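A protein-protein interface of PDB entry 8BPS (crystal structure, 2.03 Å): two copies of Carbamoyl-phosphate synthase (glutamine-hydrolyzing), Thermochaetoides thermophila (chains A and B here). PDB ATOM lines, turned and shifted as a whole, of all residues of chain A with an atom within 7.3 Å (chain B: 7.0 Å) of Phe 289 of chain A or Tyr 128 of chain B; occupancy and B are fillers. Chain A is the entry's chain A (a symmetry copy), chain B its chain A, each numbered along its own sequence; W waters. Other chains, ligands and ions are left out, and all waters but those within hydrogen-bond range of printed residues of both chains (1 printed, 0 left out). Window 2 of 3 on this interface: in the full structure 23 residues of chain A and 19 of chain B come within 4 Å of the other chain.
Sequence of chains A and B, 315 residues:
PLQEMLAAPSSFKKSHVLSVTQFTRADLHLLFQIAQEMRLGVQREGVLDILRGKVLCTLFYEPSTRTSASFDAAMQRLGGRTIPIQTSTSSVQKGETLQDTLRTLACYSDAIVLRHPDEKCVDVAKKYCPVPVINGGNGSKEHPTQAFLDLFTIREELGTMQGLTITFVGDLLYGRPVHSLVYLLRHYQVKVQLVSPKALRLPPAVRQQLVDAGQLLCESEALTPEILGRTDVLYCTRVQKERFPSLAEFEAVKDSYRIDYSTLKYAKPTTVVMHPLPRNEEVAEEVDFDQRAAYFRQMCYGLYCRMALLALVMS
NH1 of Arg 103 of chain B is in salt-bridge range of OD2 of Asp 288 of chain A (2.8 Å).
The side-chain carboxylate (OD1) of Asp 100 of chain B lies within salt-bridge range of the guanidinium group (NH2) of Arg 279 of chain A.
The backbone carbonyl oxygen (O) of Gln 99 of chain B lies within hydrogen-bond range of the guanidinium group (NE) of Arg 103 of chain B (3.0 Å).
OD1 of Asp 288 of chain A is in hydrogen-bond range of OH of Tyr 295 of chain A (2.7 Å).
The side-chain amino group of Lys 127 of chain B is in hydrogen-bond range of the side-chain hydroxyl of Tyr 128 of chain B, 2.9 Å away.
The guanidinium group (NH2) of Arg 279 of chain A lies within salt-bridge range of the side-chain carboxylate (OD2) of Asp 288 of chain A.
OD1 of Asp 100 of chain B lies within salt-bridge range of NH2 of Arg 103 of chain B (2.8 Å).
Arg 103 of chain B touches Arg 279 of chain A (NH2 to NH2, 3.5 Å).
O of Lys 127 of chain B touches CZ of Phe 289 of chain A, at 3.7 Å.
CE2 of Phe 289 of chain A touches CE1 of Tyr 128 of chain B, 3.8 Å away.
OD1 of Asp 100 of chain B touches CZ of Phe 296 of chain A (3.6 Å).
Phe 296 of chain A touches Arg 103 of chain B (CZ to NE, 3.4 Å).
Of chain B, only Lys 127 and Tyr 128 come within 4 Å of Phe 289 of chain A.
Of chain A, only Phe 289 (3.8 Å) comes within 4 Å of Tyr 128 of chain B.
Printed residues of chain A within 4 Å of Lys 127 of chain B: Phe 289 (3.7 Å).
Of the printed residues of chain B, Asp 288 of chain A touches Arg 103.
The nearest residue of chain B that does not touch Phe 289 of chain A is Arg 103 of chain B (5.2 Å).
The nearest residue of chain A that does not touch Tyr 128 of chain B is Asp 288 of chain A (4.6 Å).
The nearest printed residue of chain B that does not touch Arg 279 of chain A is Gln 99 of chain B (5.6 Å).
Printed residues of chain B that touch a printed residue of chain A: Asp 100, Arg 103, Lys 127 and Tyr 128.
Of the 14 printed residues of chain A, 4 touch a printed residue of chain B.
Printed residues of chain A that touch a printed residue of chain B: Arg 279, Asp 288, Phe 289 and Phe 296.
Hydrophobic or aromatic side chains of chain A within 4 Å of the printed part of chain B: Phe 289 and Phe 296.
Among the printed residues, Asp or Glu carboxylates within 4 Å of a Lys or Arg side-chain nitrogen of the other chain: Arg 279 of chain A with Asp 100 of chain B (2.8 Å) and Asp 288 of chain A with Arg 103 of chain B (2.8 Å).
No position is printed for both chains.
Of the 7 pairs that touch across the chains among the printed residues, none has its exchanged pair printed and touching as well.
Water W1 lies within hydrogen-bond range of the side-chain carboxylate of Asp 100 of chain B (2.6 Å) and the backbone NH of Arg 279 of chain A (3.1 Å).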
ATOM      1  N   TYR A 261      12.540   5.720 -16.918  1.00  0.00           N
ATOM      2  CA  TYR A 261      12.923   4.353 -16.570  1.00  0.00           C
ATOM      3  C   TYR A 261      14.429   4.148 -16.738  1.00  0.00           C
ATOM      4  O   TYR A 261      15.052   3.396 -15.972  1.00  0.00           O
ATOM      5  CB  TYR A 261      12.125   3.347 -17.401  1.00  0.00           C
ATOM      6  CG  TYR A 261      10.766   3.076 -16.779  1.00  0.00           C
ATOM      7  CD1 TYR A 261      10.639   2.718 -15.429  1.00  0.00           C
ATOM      8  CD2 TYR A 261       9.606   3.216 -17.525  1.00  0.00           C
ATOM      9  CE1 TYR A 261       9.388   2.501 -14.848  1.00  0.00           C
ATOM     10  CE2 TYR A 261       8.358   2.983 -16.958  1.00  0.00           C
ATOM     11  CZ  TYR A 261       8.251   2.621 -15.624  1.00  0.00           C
ATOM     12  OH  TYR A 261       6.984   2.377 -15.097  1.00  0.00           O
ATOM     13  N   ARG A 279       5.600  20.400 -13.052  1.00  0.00           N
ATOM     14  CA  ARG A 279       6.753  19.839 -13.740  1.00  0.00           C
ATOM     15  C   ARG A 279       6.718  20.193 -15.224  1.00  0.00           C
ATOM     16  O   ARG A 279       5.655  20.456 -15.795  1.00  0.00           O
ATOM     17  CB  ARG A 279       6.795  18.319 -13.567  1.00  0.00           C
ATOM     18  CG  ARG A 279       5.619  17.642 -14.230  1.00  0.00           C
ATOM     19  CD  ARG A 279       5.749  16.124 -14.179  1.00  0.00           C
ATOM     20  NE  ARG A 279       4.470  15.429 -14.283  1.00  0.00           N
ATOM     21  CZ  ARG A 279       4.343  14.136 -14.505  1.00  0.00           C
ATOM     22  NH1 ARG A 279       5.414  13.349 -14.620  1.00  0.00           N
ATOM     23  NH2 ARG A 279       3.117  13.624 -14.643  1.00  0.00           N
ATOM     24  N   ALA A 284       9.498  12.025 -16.405  1.00  0.00           N
ATOM     25  CA  ALA A 284       8.764  11.571 -17.574  1.00  0.00           C
ATOM     26  C   ALA A 284       7.423  10.945 -17.185  1.00  0.00           C
ATOM     27  O   ALA A 284       7.288  10.306 -16.135  1.00  0.00           O
ATOM     28  CB  ALA A 284       9.611  10.575 -18.362  1.00  0.00           C
ATOM     29  N   GLU A 285       6.430  11.119 -18.066  1.00  0.00           N
ATOM     30  CA  GLU A 285       5.101  10.596 -17.777  1.00  0.00           C
ATOM     31  C   GLU A 285       5.143   9.081 -17.616  1.00  0.00           C
ATOM     32  O   GLU A 285       4.324   8.514 -16.882  1.00  0.00           O
ATOM     33  CB  GLU A 285       4.098  10.973 -18.878  1.00  0.00           C
ATOM     34  N   GLU A 286       6.107   8.414 -18.280  1.00  0.00           N
ATOM     35  CA  GLU A 286       6.169   6.951 -18.257  1.00  0.00           C
ATOM     36  C   GLU A 286       6.373   6.393 -16.852  1.00  0.00           C
ATOM     37  O   GLU A 286       6.050   5.224 -16.597  1.00  0.00           O
ATOM     38  CB  GLU A 286       7.275   6.425 -19.194  1.00  0.00           C
ATOM     39  CG  GLU A 286       8.722   6.860 -18.848  1.00  0.00           C
ATOM     40  CD  GLU A 286       9.784   6.207 -19.719  1.00  0.00           C
ATOM     41  OE1 GLU A 286      10.917   5.994 -19.212  1.00  0.00           O
ATOM     42  OE2 GLU A 286       9.502   5.933 -20.912  1.00  0.00           O
ATOM     43  N   VAL A 287       6.895   7.195 -15.920  1.00  0.00           N
ATOM     44  CA  VAL A 287       7.100   6.690 -14.570  1.00  0.00           C
ATOM     45  C   VAL A 287       5.935   6.982 -13.633  1.00  0.00           C
ATOM     46  O   VAL A 287       5.956   6.509 -12.490  1.00  0.00           O
ATOM     47  CB  VAL A 287       8.423   7.234 -13.998  1.00  0.00           C
ATOM     48  CG1 VAL A 287       9.573   7.019 -15.003  1.00  0.00           C
ATOM     49  CG2 VAL A 287       8.312   8.683 -13.630  1.00  0.00           C
ATOM     50  N   ASP A 288       4.876   7.665 -14.112  1.00  0.00           N
ATOM     51  CA  ASP A 288       3.796   8.123 -13.237  1.00  0.00           C
ATOM     52  C   ASP A 288       3.108   6.971 -12.523  1.00  0.00           C
ATOM     53  O   ASP A 288       2.586   7.154 -11.417  1.00  0.00           O
ATOM     54  CB  ASP A 288       2.731   8.873 -14.050  1.00  0.00           C
ATOM     55  CG  ASP A 288       3.148  10.293 -14.431  1.00  0.00           C
ATOM     56  OD1 ASP A 288       4.276  10.748 -14.070  1.00  0.00           O
ATOM     57  OD2 ASP A 288       2.345  10.947 -15.124  1.00  0.00           O
ATOM     58  N   PHE A 289       2.992   5.817 -13.177  1.00  0.00           N
ATOM     59  CA  PHE A 289       2.323   4.679 -12.566  1.00  0.00           C
ATOM     60  C   PHE A 289       3.267   3.805 -11.766  1.00  0.00           C
ATOM     61  O   PHE A 289       2.815   2.806 -11.193  1.00  0.00           O
ATOM     62  CB  PHE A 289       1.582   3.845 -13.630  1.00  0.00           C
ATOM     63  CG  PHE A 289       0.264   4.465 -14.030  1.00  0.00           C
ATOM     64  CD1 PHE A 289      -0.846   4.380 -13.193  1.00  0.00           C
ATOM     65  CD2 PHE A 289       0.148   5.172 -15.206  1.00  0.00           C
ATOM     66  CE1 PHE A 289      -2.077   4.992 -13.556  1.00  0.00           C
ATOM     67  CE2 PHE A 289      -1.059   5.792 -15.557  1.00  0.00           C
ATOM     68  CZ  PHE A 289      -2.173   5.686 -14.732  1.00  0.00           C
ATOM     69  N   ASP A 290       4.546   4.165 -11.697  1.00  0.00           N
ATOM     70  CA  ASP A 290       5.493   3.427 -10.864  1.00  0.00           C
ATOM     71  C   ASP A 290       5.208   3.685  -9.383  1.00  0.00           C
ATOM     72  O   ASP A 290       4.942   4.821  -8.975  1.00  0.00           O
ATOM     73  CB  ASP A 290       6.923   3.856 -11.225  1.00  0.00           C
ATOM     74  CG  ASP A 290       7.996   2.928 -10.669  1.00  0.00           C
ATOM     75  OD1 ASP A 290       8.250   2.994  -9.456  1.00  0.00           O
ATOM     76  OD2 ASP A 290       8.601   2.133 -11.436  1.00  0.00           O
ATOM     77  N   GLN A 291       5.264   2.618  -8.589  1.00  0.00           N
ATOM     78  CA  GLN A 291       5.149   2.683  -7.130  1.00  0.00           C
ATOM     79  C   GLN A 291       5.918   3.864  -6.529  1.00  0.00           C
ATOM     80  O   GLN A 291       5.469   4.502  -5.567  1.00  0.00           O
ATOM     81  CB  GLN A 291       5.703   1.384  -6.485  1.00  0.00           C
ATOM     82  CG  GLN A 291       4.995   0.056  -6.788  1.00  0.00           C
ATOM     83  CD  GLN A 291       5.709  -1.228  -6.263  1.00  0.00           C
ATOM     84  OE1 GLN A 291       6.933  -1.300  -6.094  1.00  0.00           O
ATOM     85  NE2 GLN A 291       4.904  -2.246  -6.017  1.00  0.00           N
ATOM     86  N   ARG A 292       7.104   4.111  -7.045  1.00  0.00           N
ATOM     87  CA  ARG A 292       7.974   5.105  -6.455  1.00  0.00           C
ATOM     88  C   ARG A 292       7.562   6.507  -6.835  1.00  0.00           C
ATOM     89  O   ARG A 292       8.117   7.464  -6.291  1.00  0.00           O
ATOM     90  CB  ARG A 292       9.413   4.818  -6.872  1.00  0.00           C
ATOM     91  CG  ARG A 292       9.891   3.454  -6.376  1.00  0.00           C
ATOM     92  CD  ARG A 292      11.108   2.981  -7.138  1.00  0.00           C
ATOM     93  NE  ARG A 292      10.784   2.483  -8.469  1.00  0.00           N
ATOM     94  CZ  ARG A 292      11.664   1.895  -9.273  1.00  0.00           C
ATOM     95  NH1 ARG A 292      12.935   1.727  -8.911  1.00  0.00           N
ATOM     96  NH2 ARG A 292      11.261   1.469 -10.464  1.00  0.00           N
ATOM     97  N   ALA A 293       6.581   6.655  -7.723  1.00  0.00           N
ATOM     98  CA  ALA A 293       6.177   7.992  -8.177  1.00  0.00           C
ATOM     99  C   ALA A 293       5.246   8.554  -7.112  1.00  0.00           C
ATOM    100  O   ALA A 293       4.072   8.176  -7.033  1.00  0.00           O
ATOM    101  CB  ALA A 293       5.526   7.919  -9.551  1.00  0.00           C
ATOM    102  N   TYR A 295       4.780  12.021  -6.346  1.00  0.00           N
ATOM    103  CA  TYR A 295       4.436  13.447  -6.447  1.00  0.00           C
ATOM    104  C   TYR A 295       2.925  13.694  -6.475  1.00  0.00           C
ATOM    105  O   TYR A 295       2.503  14.839  -6.244  1.00  0.00           O
ATOM    106  CB  TYR A 295       5.149  14.109  -7.669  1.00  0.00           C
ATOM    107  CG  TYR A 295       5.381  13.151  -8.844  1.00  0.00           C
ATOM    108  CD1 TYR A 295       6.502  12.308  -8.881  1.00  0.00           C
ATOM    109  CD2 TYR A 295       4.470  13.085  -9.894  1.00  0.00           C
ATOM    110  CE1 TYR A 295       6.699  11.390  -9.933  1.00  0.00           C
ATOM    111  CE2 TYR A 295       4.653  12.182 -10.967  1.00  0.00           C
ATOM    112  CZ  TYR A 295       5.781  11.335 -10.975  1.00  0.00           C
ATOM    113  OH  TYR A 295       5.991  10.449 -12.005  1.00  0.00           O
ATOM    114  N   PHE A 296       2.100  12.684  -6.743  1.00  0.00           N
ATOM    115  CA  PHE A 296       0.664  12.888  -6.553  1.00  0.00           C
ATOM    116  C   PHE A 296       0.207  12.492  -5.137  1.00  0.00           C
ATOM    117  O   PHE A 296      -0.608  13.192  -4.529  1.00  0.00           O
ATOM    118  CB  PHE A 296      -0.098  12.125  -7.642  1.00  0.00           C
ATOM    119  CG  PHE A 296       0.141  12.685  -9.013  1.00  0.00           C
ATOM    120  CD1 PHE A 296      -0.254  13.968  -9.323  1.00  0.00           C
ATOM    121  CD2 PHE A 296       0.808  11.950  -9.978  1.00  0.00           C
ATOM    122  CE1 PHE A 296      -0.025  14.500 -10.598  1.00  0.00           C
ATOM    123  CE2 PHE A 296       1.028  12.464 -11.258  1.00  0.00           C
ATOM    124  CZ  PHE A 296       0.620  13.744 -11.561  1.00  0.00           C
ATOM    125  N   HIS B  16     -17.502   7.094 -14.162  1.00  0.00           N
ATOM    126  CA  HIS B  16     -17.349   8.265 -15.017  1.00  0.00           C
ATOM    127  C   HIS B  16     -18.640   8.468 -15.802  1.00  0.00           C
ATOM    128  O   HIS B  16     -19.298   7.500 -16.210  1.00  0.00           O
ATOM    129  CB  HIS B  16     -16.194   8.097 -16.008  1.00  0.00           C
ATOM    130  CG  HIS B  16     -14.838   7.942 -15.378  1.00  0.00           C
ATOM    131  ND1 HIS B  16     -14.330   8.848 -14.475  1.00  0.00           N
ATOM    132  CD2 HIS B  16     -13.874   7.000 -15.552  1.00  0.00           C
ATOM    133  CE1 HIS B  16     -13.111   8.475 -14.116  1.00  0.00           C
ATOM    134  NE2 HIS B  16     -12.811   7.351 -14.751  1.00  0.00           N
ATOM    135  N   LEU B  98      -3.510  18.499 -18.570  1.00  0.00           N
ATOM    136  CA  LEU B  98      -4.794  18.107 -17.996  1.00  0.00           C
ATOM    137  C   LEU B  98      -4.633  16.975 -16.974  1.00  0.00           C
ATOM    138  O   LEU B  98      -5.173  17.054 -15.864  1.00  0.00           O
ATOM    139  CB  LEU B  98      -5.769  17.705 -19.114  1.00  0.00           C
ATOM    140  CG  LEU B  98      -7.116  17.077 -18.695  1.00  0.00           C
ATOM    141  CD1 LEU B  98      -7.899  18.107 -17.853  1.00  0.00           C
ATOM    142  CD2 LEU B  98      -7.905  16.636 -19.932  1.00  0.00           C
ATOM    143  N   GLN B  99      -3.873  15.924 -17.326  1.00  0.00           N
ATOM    144  CA  GLN B  99      -3.758  14.764 -16.430  1.00  0.00           C
ATOM    145  C   GLN B  99      -3.087  15.135 -15.103  1.00  0.00           C
ATOM    146  O   GLN B  99      -3.448  14.590 -14.044  1.00  0.00           O
ATOM    147  CB  GLN B  99      -3.003  13.599 -17.115  1.00  0.00           C
ATOM    148  CG  GLN B  99      -1.615  13.998 -17.683  1.00  0.00           C
ATOM    149  CD  GLN B  99      -1.731  14.320 -19.164  1.00  0.00           C
ATOM    150  OE1 GLN B  99      -2.674  15.005 -19.591  1.00  0.00           O
ATOM    151  NE2 GLN B  99      -0.738  13.913 -19.941  1.00  0.00           N
ATOM    152  N   ASP B 100      -2.117  16.059 -15.129  1.00  0.00           N
ATOM    153  CA  ASP B 100      -1.504  16.516 -13.875  1.00  0.00           C
ATOM    154  C   ASP B 100      -2.536  17.247 -13.006  1.00  0.00           C
ATOM    155  O   ASP B 100      -2.649  16.999 -11.794  1.00  0.00           O
ATOM    156  CB  ASP B 100      -0.281  17.424 -14.172  1.00  0.00           C
ATOM    157  CG  ASP B 100       1.012  16.605 -14.460  1.00  0.00           C
ATOM    158  OD1 ASP B 100       0.888  15.383 -14.747  1.00  0.00           O
ATOM    159  OD2 ASP B 100       2.140  17.179 -14.415  1.00  0.00           O
ATOM    160  N   LEU B 102      -5.846  16.955 -13.102  1.00  0.00           N
ATOM    161  CA  LEU B 102      -6.880  16.046 -12.628  1.00  0.00           C
ATOM    162  C   LEU B 102      -6.383  15.229 -11.438  1.00  0.00           C
ATOM    163  O   LEU B 102      -7.087  15.075 -10.436  1.00  0.00           O
ATOM    164  CB  LEU B 102      -7.330  15.118 -13.754  1.00  0.00           C
ATOM    165  CG  LEU B 102      -8.247  15.710 -14.838  1.00  0.00           C
ATOM    166  CD1 LEU B 102      -8.414  14.656 -15.957  1.00  0.00           C
ATOM    167  CD2 LEU B 102      -9.559  16.141 -14.321  1.00  0.00           C
ATOM    168  N   ARG B 103      -5.178  14.682 -11.540  1.00  0.00           N
ATOM    169  CA  ARG B 103      -4.654  13.884 -10.448  1.00  0.00           C
ATOM    170  C   ARG B 103      -4.398  14.716  -9.208  1.00  0.00           C
ATOM    171  O   ARG B 103      -4.533  14.200  -8.092  1.00  0.00           O
ATOM    172  CB  ARG B 103      -3.386  13.185 -10.906  1.00  0.00           C
ATOM    173  CG  ARG B 103      -3.670  11.986 -11.811  1.00  0.00           C
ATOM    174  CD  ARG B 103      -2.389  11.361 -12.406  1.00  0.00           C
ATOM    175  NE  ARG B 103      -1.804  12.208 -13.428  1.00  0.00           N
ATOM    176  CZ  ARG B 103      -0.764  11.886 -14.187  1.00  0.00           C
ATOM    177  NH1 ARG B 103      -0.206  10.679 -14.130  1.00  0.00           N
ATOM    178  NH2 ARG B 103      -0.267  12.801 -15.027  1.00  0.00           N
ATOM    179  N   ALA B 106      -7.991  15.325  -7.817  1.00  0.00           N
ATOM    180  CA  ALA B 106      -8.509  14.070  -7.274  1.00  0.00           C
ATOM    181  C   ALA B 106      -8.051  13.832  -5.837  1.00  0.00           C
ATOM    182  O   ALA B 106      -8.703  13.072  -5.111  1.00  0.00           O
ATOM    183  CB  ALA B 106      -8.066  12.887  -8.141  1.00  0.00           C
ATOM    184  N   ASP B 123     -10.739  10.805 -22.736  1.00  0.00           N
ATOM    185  CA  ASP B 123      -9.809   9.679 -22.728  1.00  0.00           C
ATOM    186  C   ASP B 123      -8.679   9.920 -21.737  1.00  0.00           C
ATOM    187  O   ASP B 123      -8.249   9.002 -21.041  1.00  0.00           O
ATOM    188  CB  ASP B 123      -9.264   9.469 -24.139  1.00  0.00           C
ATOM    189  CG  ASP B 123     -10.377   9.179 -25.139  1.00  0.00           C
ATOM    190  OD1 ASP B 123     -10.251   9.631 -26.302  1.00  0.00           O
ATOM    191  OD2 ASP B 123     -11.385   8.519 -24.760  1.00  0.00           O
ATOM    192  N   VAL B 124      -8.199  11.161 -21.644  1.00  0.00           N
ATOM    193  CA  VAL B 124      -7.220  11.502 -20.620  1.00  0.00           C
ATOM    194  C   VAL B 124      -7.784  11.230 -19.228  1.00  0.00           C
ATOM    195  O   VAL B 124      -7.110  10.634 -18.372  1.00  0.00           O
ATOM    196  CB  VAL B 124      -6.797  12.970 -20.765  1.00  0.00           C
ATOM    197  CG1 VAL B 124      -5.944  13.372 -19.580  1.00  0.00           C
ATOM    198  CG2 VAL B 124      -6.089  13.149 -22.090  1.00  0.00           C
ATOM    199  N   ALA B 125      -9.025  11.685 -18.975  1.00  0.00           N
ATOM    200  CA  ALA B 125      -9.656  11.446 -17.685  1.00  0.00           C
ATOM    201  C   ALA B 125      -9.757   9.957 -17.379  1.00  0.00           C
ATOM    202  O   ALA B 125      -9.463   9.526 -16.255  1.00  0.00           O
ATOM    203  CB  ALA B 125     -11.051  12.081 -17.654  1.00  0.00           C
ATOM    204  N   LYS B 126     -10.163   9.158 -18.362  1.00  0.00           N
ATOM    205  CA  LYS B 126     -10.286   7.724 -18.139  1.00  0.00           C
ATOM    206  C   LYS B 126      -8.955   7.112 -17.732  1.00  0.00           C
ATOM    207  O   LYS B 126      -8.878   6.315 -16.795  1.00  0.00           O
ATOM    208  CB  LYS B 126     -10.784   7.029 -19.403  1.00  0.00           C
ATOM    209  CG  LYS B 126     -12.255   6.827 -19.475  1.00  0.00           C
ATOM    210  CD  LYS B 126     -12.777   6.931 -20.914  1.00  0.00           C
ATOM    211  CE  LYS B 126     -12.065   5.997 -21.879  1.00  0.00           C
ATOM    212  NZ  LYS B 126     -13.026   5.565 -22.969  1.00  0.00           N
ATOM    213  N   LYS B 127      -7.907   7.417 -18.485  1.00  0.00           N
ATOM    214  CA  LYS B 127      -6.598   6.812 -18.236  1.00  0.00           C
ATOM    215  C   LYS B 127      -6.037   7.207 -16.876  1.00  0.00           C
ATOM    216  O   LYS B 127      -5.466   6.372 -16.161  1.00  0.00           O
ATOM    217  CB  LYS B 127      -5.637   7.241 -19.341  1.00  0.00           C
ATOM    218  CG  LYS B 127      -4.187   6.770 -19.210  1.00  0.00           C
ATOM    219  CD  LYS B 127      -3.549   6.732 -20.584  1.00  0.00           C
ATOM    220  CE  LYS B 127      -2.028   6.694 -20.523  1.00  0.00           C
ATOM    221  NZ  LYS B 127      -1.445   7.617 -21.550  1.00  0.00           N
ATOM    222  N   TYR B 128      -6.198   8.462 -16.488  1.00  0.00           N
ATOM    223  CA  TYR B 128      -5.433   8.971 -15.365  1.00  0.00           C
ATOM    224  C   TYR B 128      -6.230   9.298 -14.111  1.00  0.00           C
ATOM    225  O   TYR B 128      -5.647   9.270 -13.025  1.00  0.00           O
ATOM    226  CB  TYR B 128      -4.682  10.244 -15.777  1.00  0.00           C
ATOM    227  CG  TYR B 128      -3.577  10.014 -16.769  1.00  0.00           C
ATOM    228  CD1 TYR B 128      -2.396   9.396 -16.378  1.00  0.00           C
ATOM    229  CD2 TYR B 128      -3.706  10.417 -18.086  1.00  0.00           C
ATOM    230  CE1 TYR B 128      -1.366   9.186 -17.281  1.00  0.00           C
ATOM    231  CE2 TYR B 128      -2.674  10.237 -18.993  1.00  0.00           C
ATOM    232  CZ  TYR B 128      -1.514   9.613 -18.587  1.00  0.00           C
ATOM    233  OH  TYR B 128      -0.494   9.400 -19.484  1.00  0.00           O
ATOM    234  N   CYS B 129      -7.501   9.677 -14.208  1.00  0.00           N
ATOM    235  CA  CYS B 129      -8.139  10.264 -13.061  1.00  0.00           C
ATOM    236  C   CYS B 129      -8.675   9.188 -12.138  1.00  0.00           C
ATOM    237  O   CYS B 129      -9.572   8.445 -12.540  1.00  0.00           O
ATOM    238  CB  CYS B 129      -9.270  11.171 -13.488  1.00  0.00           C
ATOM    239  SG  CYS B 129      -9.869  12.151 -12.086  1.00  0.00           S
ATOM    240  N   PRO B 130      -8.232   9.121 -10.883  1.00  0.00           N
ATOM    241  CA  PRO B 130      -8.706   8.059  -9.983  1.00  0.00           C
ATOM    242  C   PRO B 130     -10.012   8.367  -9.268  1.00  0.00           C
ATOM    243  O   PRO B 130     -10.362   7.608  -8.368  1.00  0.00           O
ATOM    244  CB  PRO B 130      -7.543   7.932  -8.971  1.00  0.00           C
ATOM    245  CG  PRO B 130      -7.066   9.429  -8.813  1.00  0.00           C
ATOM    246  CD  PRO B 130      -7.240  10.018 -10.237  1.00  0.00           C
ATOM    247  N   VAL B 131     -10.727   9.446  -9.589  1.00  0.00           N
ATOM    248  CA  VAL B 131     -12.082   9.643  -9.070  1.00  0.00           C
ATOM    249  C   VAL B 131     -13.014   9.834 -10.249  1.00  0.00           C
ATOM    250  O   VAL B 131     -12.570  10.174 -11.365  1.00  0.00           O
ATOM    251  CB  VAL B 131     -12.181  10.863  -8.117  1.00  0.00           C
ATOM    252  CG1 VAL B 131     -11.336  10.712  -6.854  1.00  0.00           C
ATOM    253  CG2 VAL B 131     -11.870  12.221  -8.880  1.00  0.00           C
HETATM  254  O   HOH W   1       2.652  19.596 -13.640  1.00  0.00           O
